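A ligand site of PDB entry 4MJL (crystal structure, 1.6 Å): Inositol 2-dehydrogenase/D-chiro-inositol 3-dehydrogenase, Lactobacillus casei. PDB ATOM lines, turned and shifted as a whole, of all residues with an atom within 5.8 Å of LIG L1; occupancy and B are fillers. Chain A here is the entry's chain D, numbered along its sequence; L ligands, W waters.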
ATOM      1  N   LYS A 109       7.973 -11.055  -3.638  1.00  0.00           N
ATOM      2  CA  LYS A 109       6.802 -11.134  -4.482  1.00  0.00           C
ATOM      3  C   LYS A 109       5.655 -11.918  -3.777  1.00  0.00           C
ATOM      4  O   LYS A 109       5.891 -12.657  -2.837  1.00  0.00           O
ATOM      5  CB  LYS A 109       7.163 -11.686  -5.866  1.00  0.00           C
ATOM      6  CG  LYS A 109       8.055 -12.929  -5.931  1.00  0.00           C
ATOM      7  CD  LYS A 109       7.612 -14.066  -5.097  1.00  0.00           C
ATOM      8  CE  LYS A 109       6.294 -14.644  -5.523  1.00  0.00           C
ATOM      9  NZ  LYS A 109       5.987 -15.788  -4.561  1.00  0.00           N
ATOM     10  N   MET A 138      13.345 -12.682  -8.310  1.00  0.00           N
ATOM     11  CA  MET A 138      14.741 -13.079  -8.409  1.00  0.00           C
ATOM     12  C   MET A 138      15.102 -13.782  -9.713  1.00  0.00           C
ATOM     13  O   MET A 138      16.306 -13.926  -9.990  1.00  0.00           O
ATOM     14  CB  MET A 138      15.133 -14.040  -7.246  1.00  0.00           C
ATOM     15  CG  MET A 138      14.735 -15.486  -7.458  1.00  0.00           C
ATOM     16  SD  MET A 138      12.978 -15.724  -7.519  1.00  0.00           S
ATOM     17  CE  MET A 138      12.930 -17.493  -7.787  1.00  0.00           C
ATOM     18  N   ARG A 139      14.113 -14.229 -10.498  1.00  0.00           N
ATOM     19  CA  ARG A 139      14.430 -15.003 -11.719  1.00  0.00           C
ATOM     20  C   ARG A 139      15.369 -14.194 -12.632  1.00  0.00           C
ATOM     21  O   ARG A 139      16.228 -14.770 -13.299  1.00  0.00           O
ATOM     22  CB  ARG A 139      13.149 -15.344 -12.500  1.00  0.00           C
ATOM     23  CG  ARG A 139      12.138 -16.287 -11.783  1.00  0.00           C
ATOM     24  CD  ARG A 139      12.562 -17.727 -11.879  1.00  0.00           C
ATOM     25  NE  ARG A 139      11.543 -18.588 -11.313  1.00  0.00           N
ATOM     26  CZ  ARG A 139      10.503 -19.076 -11.995  1.00  0.00           C
ATOM     27  NH1 ARG A 139      10.366 -18.774 -13.273  1.00  0.00           N
ATOM     28  NH2 ARG A 139       9.606 -19.845 -11.394  1.00  0.00           N
ATOM     29  N   HIS A 167       6.642 -24.558 -14.120  1.00  0.00           N
ATOM     30  CA  HIS A 167       6.910 -24.155 -12.757  1.00  0.00           C
ATOM     31  C   HIS A 167       6.331 -25.270 -11.856  1.00  0.00           C
ATOM     32  O   HIS A 167       5.131 -25.433 -11.708  1.00  0.00           O
ATOM     33  CB  HIS A 167       6.222 -22.833 -12.515  1.00  0.00           C
ATOM     34  CG  HIS A 167       6.627 -22.177 -11.246  1.00  0.00           C
ATOM     35  ND1 HIS A 167       6.451 -20.832 -11.032  1.00  0.00           N
ATOM     36  CD2 HIS A 167       7.252 -22.658 -10.154  1.00  0.00           C
ATOM     37  CE1 HIS A 167       6.910 -20.522  -9.839  1.00  0.00           C
ATOM     38  NE2 HIS A 167       7.389 -21.612  -9.272  1.00  0.00           N
ATOM     39  N   ILE A 168       7.252 -26.081 -11.333  1.00  0.00           N
ATOM     40  CA  ILE A 168       6.894 -27.325 -10.674  1.00  0.00           C
ATOM     41  C   ILE A 168       7.257 -27.226  -9.190  1.00  0.00           C
ATOM     42  O   ILE A 168       8.359 -26.813  -8.848  1.00  0.00           O
ATOM     43  CB  ILE A 168       7.709 -28.490 -11.275  1.00  0.00           C
ATOM     44  CG1 ILE A 168       7.572 -28.596 -12.808  1.00  0.00           C
ATOM     45  CG2 ILE A 168       7.356 -29.780 -10.573  1.00  0.00           C
ATOM     46  CD1 ILE A 168       6.206 -28.668 -13.315  1.00  0.00           C
ATOM     47  N   ASN A 169       6.323 -27.592  -8.315  1.00  0.00           N
ATOM     48  CA  ASN A 169       6.608 -27.664  -6.868  1.00  0.00           C
ATOM     49  C   ASN A 169       6.132 -29.021  -6.434  1.00  0.00           C
ATOM     50  O   ASN A 169       5.190 -29.524  -7.003  1.00  0.00           O
ATOM     51  CB  ASN A 169       5.781 -26.681  -6.034  1.00  0.00           C
ATOM     52  CG  ASN A 169       6.023 -25.232  -6.337  1.00  0.00           C
ATOM     53  OD1 ASN A 169       6.914 -24.802  -7.111  1.00  0.00           O
ATOM     54  ND2 ASN A 169       5.255 -24.452  -5.653  1.00  0.00           N
ATOM     55  N   TYR A 176      -2.331 -22.572   0.946  1.00  0.00           N
ATOM     56  CA  TYR A 176      -2.183 -22.264  -0.472  1.00  0.00           C
ATOM     57  C   TYR A 176      -3.551 -22.380  -1.189  1.00  0.00           C
ATOM     58  O   TYR A 176      -4.168 -23.437  -1.182  1.00  0.00           O
ATOM     59  CB  TYR A 176      -1.159 -23.194  -1.086  1.00  0.00           C
ATOM     60  CG  TYR A 176      -0.674 -22.821  -2.482  1.00  0.00           C
ATOM     61  CD1 TYR A 176      -1.454 -23.141  -3.615  1.00  0.00           C
ATOM     62  CD2 TYR A 176       0.578 -22.216  -2.686  1.00  0.00           C
ATOM     63  CE1 TYR A 176      -1.007 -22.844  -4.888  1.00  0.00           C
ATOM     64  CE2 TYR A 176       1.036 -21.902  -4.013  1.00  0.00           C
ATOM     65  CZ  TYR A 176       0.242 -22.245  -5.080  1.00  0.00           C
ATOM     66  OH  TYR A 176       0.642 -22.011  -6.359  1.00  0.00           O
ATOM     67  N   ASP A 184       1.216 -16.321  -6.250  1.00  0.00           N
ATOM     68  CA  ASP A 184       2.414 -16.812  -5.529  1.00  0.00           C
ATOM     69  C   ASP A 184       3.357 -17.509  -6.486  1.00  0.00           C
ATOM     70  O   ASP A 184       4.574 -17.507  -6.299  1.00  0.00           O
ATOM     71  CB  ASP A 184       1.997 -17.810  -4.428  1.00  0.00           C
ATOM     72  CG  ASP A 184       2.796 -17.637  -3.158  1.00  0.00           C
ATOM     73  OD1 ASP A 184       2.953 -16.491  -2.654  1.00  0.00           O
ATOM     74  OD2 ASP A 184       3.213 -18.678  -2.627  1.00  0.00           O
ATOM     75  N   THR A 185       2.783 -18.131  -7.519  1.00  0.00           N
ATOM     76  CA  THR A 185       3.562 -19.058  -8.355  1.00  0.00           C
ATOM     77  C   THR A 185       3.756 -18.509  -9.752  1.00  0.00           C
ATOM     78  O   THR A 185       4.877 -18.162 -10.135  1.00  0.00           O
ATOM     79  CB  THR A 185       2.930 -20.453  -8.318  1.00  0.00           C
ATOM     80  OG1 THR A 185       2.941 -20.881  -6.962  1.00  0.00           O
ATOM     81  CG2 THR A 185       3.732 -21.463  -9.131  1.00  0.00           C
ATOM     82  N   ILE A 187       3.194 -15.717 -10.938  1.00  0.00           N
ATOM     83  CA  ILE A 187       3.734 -14.363 -10.877  1.00  0.00           C
ATOM     84  C   ILE A 187       5.214 -14.311 -11.324  1.00  0.00           C
ATOM     85  O   ILE A 187       5.632 -13.351 -11.959  1.00  0.00           O
ATOM     86  CB  ILE A 187       3.523 -13.699  -9.489  1.00  0.00           C
ATOM     87  CG1 ILE A 187       3.590 -12.171  -9.617  1.00  0.00           C
ATOM     88  CG2 ILE A 187       4.541 -14.187  -8.478  1.00  0.00           C
ATOM     89  CD1 ILE A 187       2.272 -11.523 -10.049  1.00  0.00           C
ATOM     90  N   HIS A 188       6.007 -15.333 -11.012  1.00  0.00           N
ATOM     91  CA  HIS A 188       7.403 -15.351 -11.462  1.00  0.00           C
ATOM     92  C   HIS A 188       7.514 -15.362 -12.978  1.00  0.00           C
ATOM     93  O   HIS A 188       8.313 -14.647 -13.554  1.00  0.00           O
ATOM     94  CB  HIS A 188       8.098 -16.590 -10.929  1.00  0.00           C
ATOM     95  CG  HIS A 188       8.428 -16.507  -9.471  1.00  0.00           C
ATOM     96  ND1 HIS A 188       9.410 -15.692  -8.996  1.00  0.00           N
ATOM     97  CD2 HIS A 188       7.886 -17.151  -8.419  1.00  0.00           C
ATOM     98  CE1 HIS A 188       9.487 -15.848  -7.679  1.00  0.00           C
ATOM     99  NE2 HIS A 188       8.558 -16.710  -7.308  1.00  0.00           N
ATOM    100  N   VAL A 242       1.818 -27.630  -8.850  1.00  0.00           N
ATOM    101  CA  VAL A 242       2.355 -27.383  -7.517  1.00  0.00           C
ATOM    102  C   VAL A 242       2.161 -28.586  -6.550  1.00  0.00           C
ATOM    103  O   VAL A 242       2.573 -28.504  -5.379  1.00  0.00           O
ATOM    104  CB  VAL A 242       1.781 -26.065  -6.897  1.00  0.00           C
ATOM    105  CG1 VAL A 242       2.152 -24.895  -7.794  1.00  0.00           C
ATOM    106  CG2 VAL A 242       0.283 -26.175  -6.682  1.00  0.00           C
ATOM    107  N   TYR A 248      11.129 -29.946  -7.137  1.00  0.00           N
ATOM    108  CA  TYR A 248      10.930 -28.530  -7.420  1.00  0.00           C
ATOM    109  C   TYR A 248      11.721 -28.238  -8.672  1.00  0.00           C
ATOM    110  O   TYR A 248      12.904 -28.551  -8.745  1.00  0.00           O
ATOM    111  CB  TYR A 248      11.506 -27.715  -6.273  1.00  0.00           C
ATOM    112  CG  TYR A 248      11.355 -26.248  -6.515  1.00  0.00           C
ATOM    113  CD1 TYR A 248      12.328 -25.518  -7.243  1.00  0.00           C
ATOM    114  CD2 TYR A 248      10.212 -25.580  -6.028  1.00  0.00           C
ATOM    115  CE1 TYR A 248      12.166 -24.164  -7.488  1.00  0.00           C
ATOM    116  CE2 TYR A 248      10.068 -24.197  -6.270  1.00  0.00           C
ATOM    117  CZ  TYR A 248      11.052 -23.530  -6.977  1.00  0.00           C
ATOM    118  OH  TYR A 248      10.877 -22.198  -7.237  1.00  0.00           O
ATOM    119  N   TRP A 286      12.765 -24.272  -3.555  1.00  0.00           N
ATOM    120  CA  TRP A 286      13.352 -23.046  -4.094  1.00  0.00           C
ATOM    121  C   TRP A 286      14.581 -22.627  -3.340  1.00  0.00           C
ATOM    122  O   TRP A 286      15.419 -21.916  -3.865  1.00  0.00           O
ATOM    123  CB  TRP A 286      12.299 -21.891  -4.016  1.00  0.00           C
ATOM    124  CG  TRP A 286      11.535 -21.907  -2.755  1.00  0.00           C
ATOM    125  CD1 TRP A 286      10.368 -22.589  -2.514  1.00  0.00           C
ATOM    126  CD2 TRP A 286      11.926 -21.315  -1.498  1.00  0.00           C
ATOM    127  NE1 TRP A 286      10.012 -22.451  -1.183  1.00  0.00           N
ATOM    128  CE2 TRP A 286      10.938 -21.687  -0.545  1.00  0.00           C
ATOM    129  CE3 TRP A 286      13.011 -20.548  -1.081  1.00  0.00           C
ATOM    130  CZ2 TRP A 286      11.014 -21.259   0.812  1.00  0.00           C
ATOM    131  CZ3 TRP A 286      13.090 -20.128   0.265  1.00  0.00           C
ATOM    132  CH2 TRP A 286      12.097 -20.482   1.176  1.00  0.00           C
ATOM    133  N   PHE A 290      17.423 -21.562  -6.076  1.00  0.00           N
ATOM    134  CA  PHE A 290      17.601 -20.152  -6.443  1.00  0.00           C
ATOM    135  C   PHE A 290      18.479 -19.398  -5.455  1.00  0.00           C
ATOM    136  O   PHE A 290      18.453 -18.160  -5.413  1.00  0.00           O
ATOM    137  CB  PHE A 290      16.277 -19.431  -6.659  1.00  0.00           C
ATOM    138  CG  PHE A 290      15.592 -19.813  -7.942  1.00  0.00           C
ATOM    139  CD1 PHE A 290      16.161 -19.451  -9.161  1.00  0.00           C
ATOM    140  CD2 PHE A 290      14.435 -20.576  -7.927  1.00  0.00           C
ATOM    141  CE1 PHE A 290      15.568 -19.858 -10.371  1.00  0.00           C
ATOM    142  CE2 PHE A 290      13.809 -20.983  -9.147  1.00  0.00           C
ATOM    143  CZ  PHE A 290      14.395 -20.592 -10.363  1.00  0.00           C
ATOM    144  N   TYR A 294      18.840 -15.287  -5.174  1.00  0.00           N
ATOM    145  CA  TYR A 294      18.456 -14.553  -3.935  1.00  0.00           C
ATOM    146  C   TYR A 294      19.653 -13.766  -3.391  1.00  0.00           C
ATOM    147  O   TYR A 294      19.503 -12.621  -2.990  1.00  0.00           O
ATOM    148  CB  TYR A 294      17.966 -15.508  -2.851  1.00  0.00           C
ATOM    149  CG  TYR A 294      16.764 -16.318  -3.220  1.00  0.00           C
ATOM    150  CD1 TYR A 294      15.639 -15.734  -3.805  1.00  0.00           C
ATOM    151  CD2 TYR A 294      16.750 -17.675  -2.973  1.00  0.00           C
ATOM    152  CE1 TYR A 294      14.520 -16.515  -4.150  1.00  0.00           C
ATOM    153  CE2 TYR A 294      15.661 -18.463  -3.295  1.00  0.00           C
ATOM    154  CZ  TYR A 294      14.570 -17.891  -3.934  1.00  0.00           C
ATOM    155  OH  TYR A 294      13.496 -18.720  -4.248  1.00  0.00           O
HETATM  156  C1  LIG L   1       6.283 -21.245  -5.238  1.00  0.00           C
HETATM  157  C2  LIG L   1       7.479 -20.679  -6.103  1.00  0.00           C
HETATM  158  C3  LIG L   1       8.580 -19.913  -5.189  1.00  0.00           C
HETATM  159  C4  LIG L   1       7.836 -18.765  -4.312  1.00  0.00           C
HETATM  160  C5  LIG L   1       6.744 -19.623  -3.529  1.00  0.00           C
HETATM  161  C6  LIG L   1       5.542 -20.146  -4.352  1.00  0.00           C
HETATM  162  O1  LIG L   1       5.349 -21.790  -6.088  1.00  0.00           O
HETATM  163  O2  LIG L   1       8.175 -21.688  -6.727  1.00  0.00           O
HETATM  164  O3  LIG L   1       9.512 -19.320  -6.040  1.00  0.00           O
HETATM  165  O4  LIG L   1       7.226 -17.877  -5.160  1.00  0.00           O
HETATM  166  O5  LIG L   1       4.629 -20.776  -3.505  1.00  0.00           O
HETATM  167  O6  LIG L   1       7.015 -20.455  -2.485  1.00  0.00           O
HETATM  168  P1  LG2 L   2       5.906 -19.035   5.489  1.00  0.00           P
HETATM  169  O1  LG2 L   2       4.562 -19.463   5.656  1.00  0.00           O
HETATM  170  O2  LG2 L   2       6.873 -20.016   5.825  1.00  0.00           O
HETATM  171  O3  LG2 L   2       6.206 -17.761   6.332  1.00  0.00           O
HETATM  172  C1  LG2 L   2       5.353 -16.672   6.348  1.00  0.00           C
HETATM  173  C2  LG2 L   2       5.540 -15.979   7.676  1.00  0.00           C
HETATM  174  O4  LG2 L   2       4.844 -14.796   7.656  1.00  0.00           O
HETATM  175  C3  LG2 L   2       4.976 -16.770   8.844  1.00  0.00           C
HETATM  176  O5  LG2 L   2       5.957 -16.922   9.874  1.00  0.00           O
HETATM  177  C4  LG2 L   2       3.747 -15.999   9.258  1.00  0.00           C
HETATM  178  O6  LG2 L   2       3.413 -16.165  10.615  1.00  0.00           O
HETATM  179  C5  LG2 L   2       4.186 -14.595   8.886  1.00  0.00           C
HETATM  180  N1  LG2 L   2       3.150 -13.577   8.753  1.00  0.00           N
HETATM  181  C6  LG2 L   2       1.975 -13.702   8.155  1.00  0.00           C
HETATM  182  N2  LG2 L   2       1.306 -12.556   8.126  1.00  0.00           N
HETATM  183  C7  LG2 L   2       2.097 -11.674   8.691  1.00  0.00           C
HETATM  184  C8  LG2 L   2       1.994 -10.261   8.978  1.00  0.00           C
HETATM  185  N3  LG2 L   2       0.876  -9.624   8.644  1.00  0.00           N
HETATM  186  N4  LG2 L   2       3.031  -9.723   9.570  1.00  0.00           N
HETATM  187  C9  LG2 L   2       4.079 -10.395   9.898  1.00  0.00           C
HETATM  188  N5  LG2 L   2       4.270 -11.662   9.678  1.00  0.00           N
HETATM  189  C10 LG2 L   2       3.307 -12.336   9.099  1.00  0.00           C
HETATM  190  O7  LG2 L   2       6.037 -18.576   4.003  1.00  0.00           O
HETATM  191  P2  LG2 L   2       7.332 -18.256   3.192  1.00  0.00           P
HETATM  192  O8  LG2 L   2       7.570 -19.298   2.270  1.00  0.00           O
HETATM  193  O9  LG2 L   2       8.390 -17.766   4.011  1.00  0.00           O
HETATM  194  O10 LG2 L   2       6.772 -17.110   2.300  1.00  0.00           O
HETATM  195  C11 LG2 L   2       6.822 -15.773   2.662  1.00  0.00           C
HETATM  196  C12 LG2 L   2       6.775 -14.830   1.456  1.00  0.00           C
HETATM  197  O11 LG2 L   2       7.920 -15.086   0.685  1.00  0.00           O
HETATM  198  C13 LG2 L   2       5.648 -15.096   0.490  1.00  0.00           C
HETATM  199  O12 LG2 L   2       5.283 -13.858  -0.057  1.00  0.00           O
HETATM  200  C14 LG2 L   2       6.264 -15.950  -0.582  1.00  0.00           C
HETATM  201  O13 LG2 L   2       5.607 -15.713  -1.822  1.00  0.00           O
HETATM  202  C15 LG2 L   2       7.648 -15.373  -0.645  1.00  0.00           C
HETATM  203  N6  LG2 L   2       8.587 -16.321  -1.236  1.00  0.00           N
HETATM  204  C16 LG2 L   2       9.263 -16.014  -2.311  1.00  0.00           C
HETATM  205  C17 LG2 L   2      10.132 -16.914  -2.852  1.00  0.00           C
HETATM  206  C18 LG2 L   2      10.854 -16.585  -4.098  1.00  0.00           C
HETATM  207  O14 LG2 L   2      11.324 -17.503  -4.696  1.00  0.00           O
HETATM  208  N7  LG2 L   2      10.904 -15.318  -4.403  1.00  0.00           N
HETATM  209  C19 LG2 L   2      10.327 -18.144  -2.246  1.00  0.00           C
HETATM  210  C20 LG2 L   2       9.643 -18.439  -1.102  1.00  0.00           C
HETATM  211  C21 LG2 L   2       8.780 -17.488  -0.641  1.00  0.00           C
HETATM  212  O   HOH W   1      10.592 -19.863  -8.676  1.00  0.00           O
HETATM  213  O   HOH W   2       4.632 -22.881  -1.898  1.00  0.00           O
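Water W1 lies within hydrogen-bond range of OH of Tyr 248, NH2 of Arg 139 and O3 of LIG L1.
O14 of LG2 L2 is in hydrogen-bond range of O3 of LIG L1.
An oxygen (O4) of LIG L1 sits at hydrogen-bond distance from the side-chain amino group of Lys 109 (2.5 Å).
NE2 of His 167 is in hydrogen-bond range of O2 of LIG L1 (2.7 Å).
An oxygen (O4) of LIG L1 sits at hydrogen-bond distance from the backbone carbonyl oxygen (O) of Asp 184, at 2.9 Å.
An oxygen (O5) of LIG L1 sits at hydrogen-bond distance from the side-chain carboxylate of Asp 184, 2.7 Å away.
The side-chain amide nitrogen (ND2) of Asn 169 lies within hydrogen-bond range of an oxygen (O1) of LIG L1 (2.7 Å).
O1 of LIG L1 lies within hydrogen-bond range of OG1 of Thr 185.
O4 of LIG L1 sits at hydrogen-bond distance from NE2 of His 188 (2.8 Å).
The side-chain hydroxyl (OH) of Tyr 248 is in hydrogen-bond range of an oxygen (O2) of LIG L1 (2.8 Å).
The backbone carbonyl oxygen of Lys 109 sits at hydrogen-bond distance from an oxygen (O12) of LG2 L2, 3.1 Å away.
NZ of Lys 109 sits at hydrogen-bond distance from O13 of LG2 L2.
The side-chain carboxylate (OD1) of Asp 184 sits at hydrogen-bond distance from an oxygen (O13) of LG2 L2, at 2.9 Å.
SD of Met 138 lies within hydrogen-bond range of N7 of LG2 L2 (3.8 Å).
OH of Tyr 294 lies within hydrogen-bond range of O14 of LG2 L2 (2.5 Å).
The side-chain amino group (NZ) of Lys 109 lies within salt-bridge range of the side-chain carboxylate (OD1) of Asp 184.
O of Thr 185 lies close to ND1 of His 167 (3.2 Å).
ND1 of His 167 sits close to NH2 of Arg 139 (3.3 Å).
The side-chain hydroxyl (OG1) of Thr 185 is in hydrogen-bond range of the side-chain hydroxyl (OH) of Tyr 176.
CE2 of Tyr 176 touches O5 of LIG L1, at 3.8 Å.
Trp 286 touches LIG L1 (NE1 to O6, 3.8 Å).
Hydrophobic or aromatic side chains within 4 Å of LIG L1: His 167, Tyr 176, His 188, Tyr 248 and Trp 286.
Within 4 Å of LIG L1: Lys 109, His 167, Asn 169, Tyr 176, Asp 184, Thr 185, His 188, Tyr 248 and Trp 286.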
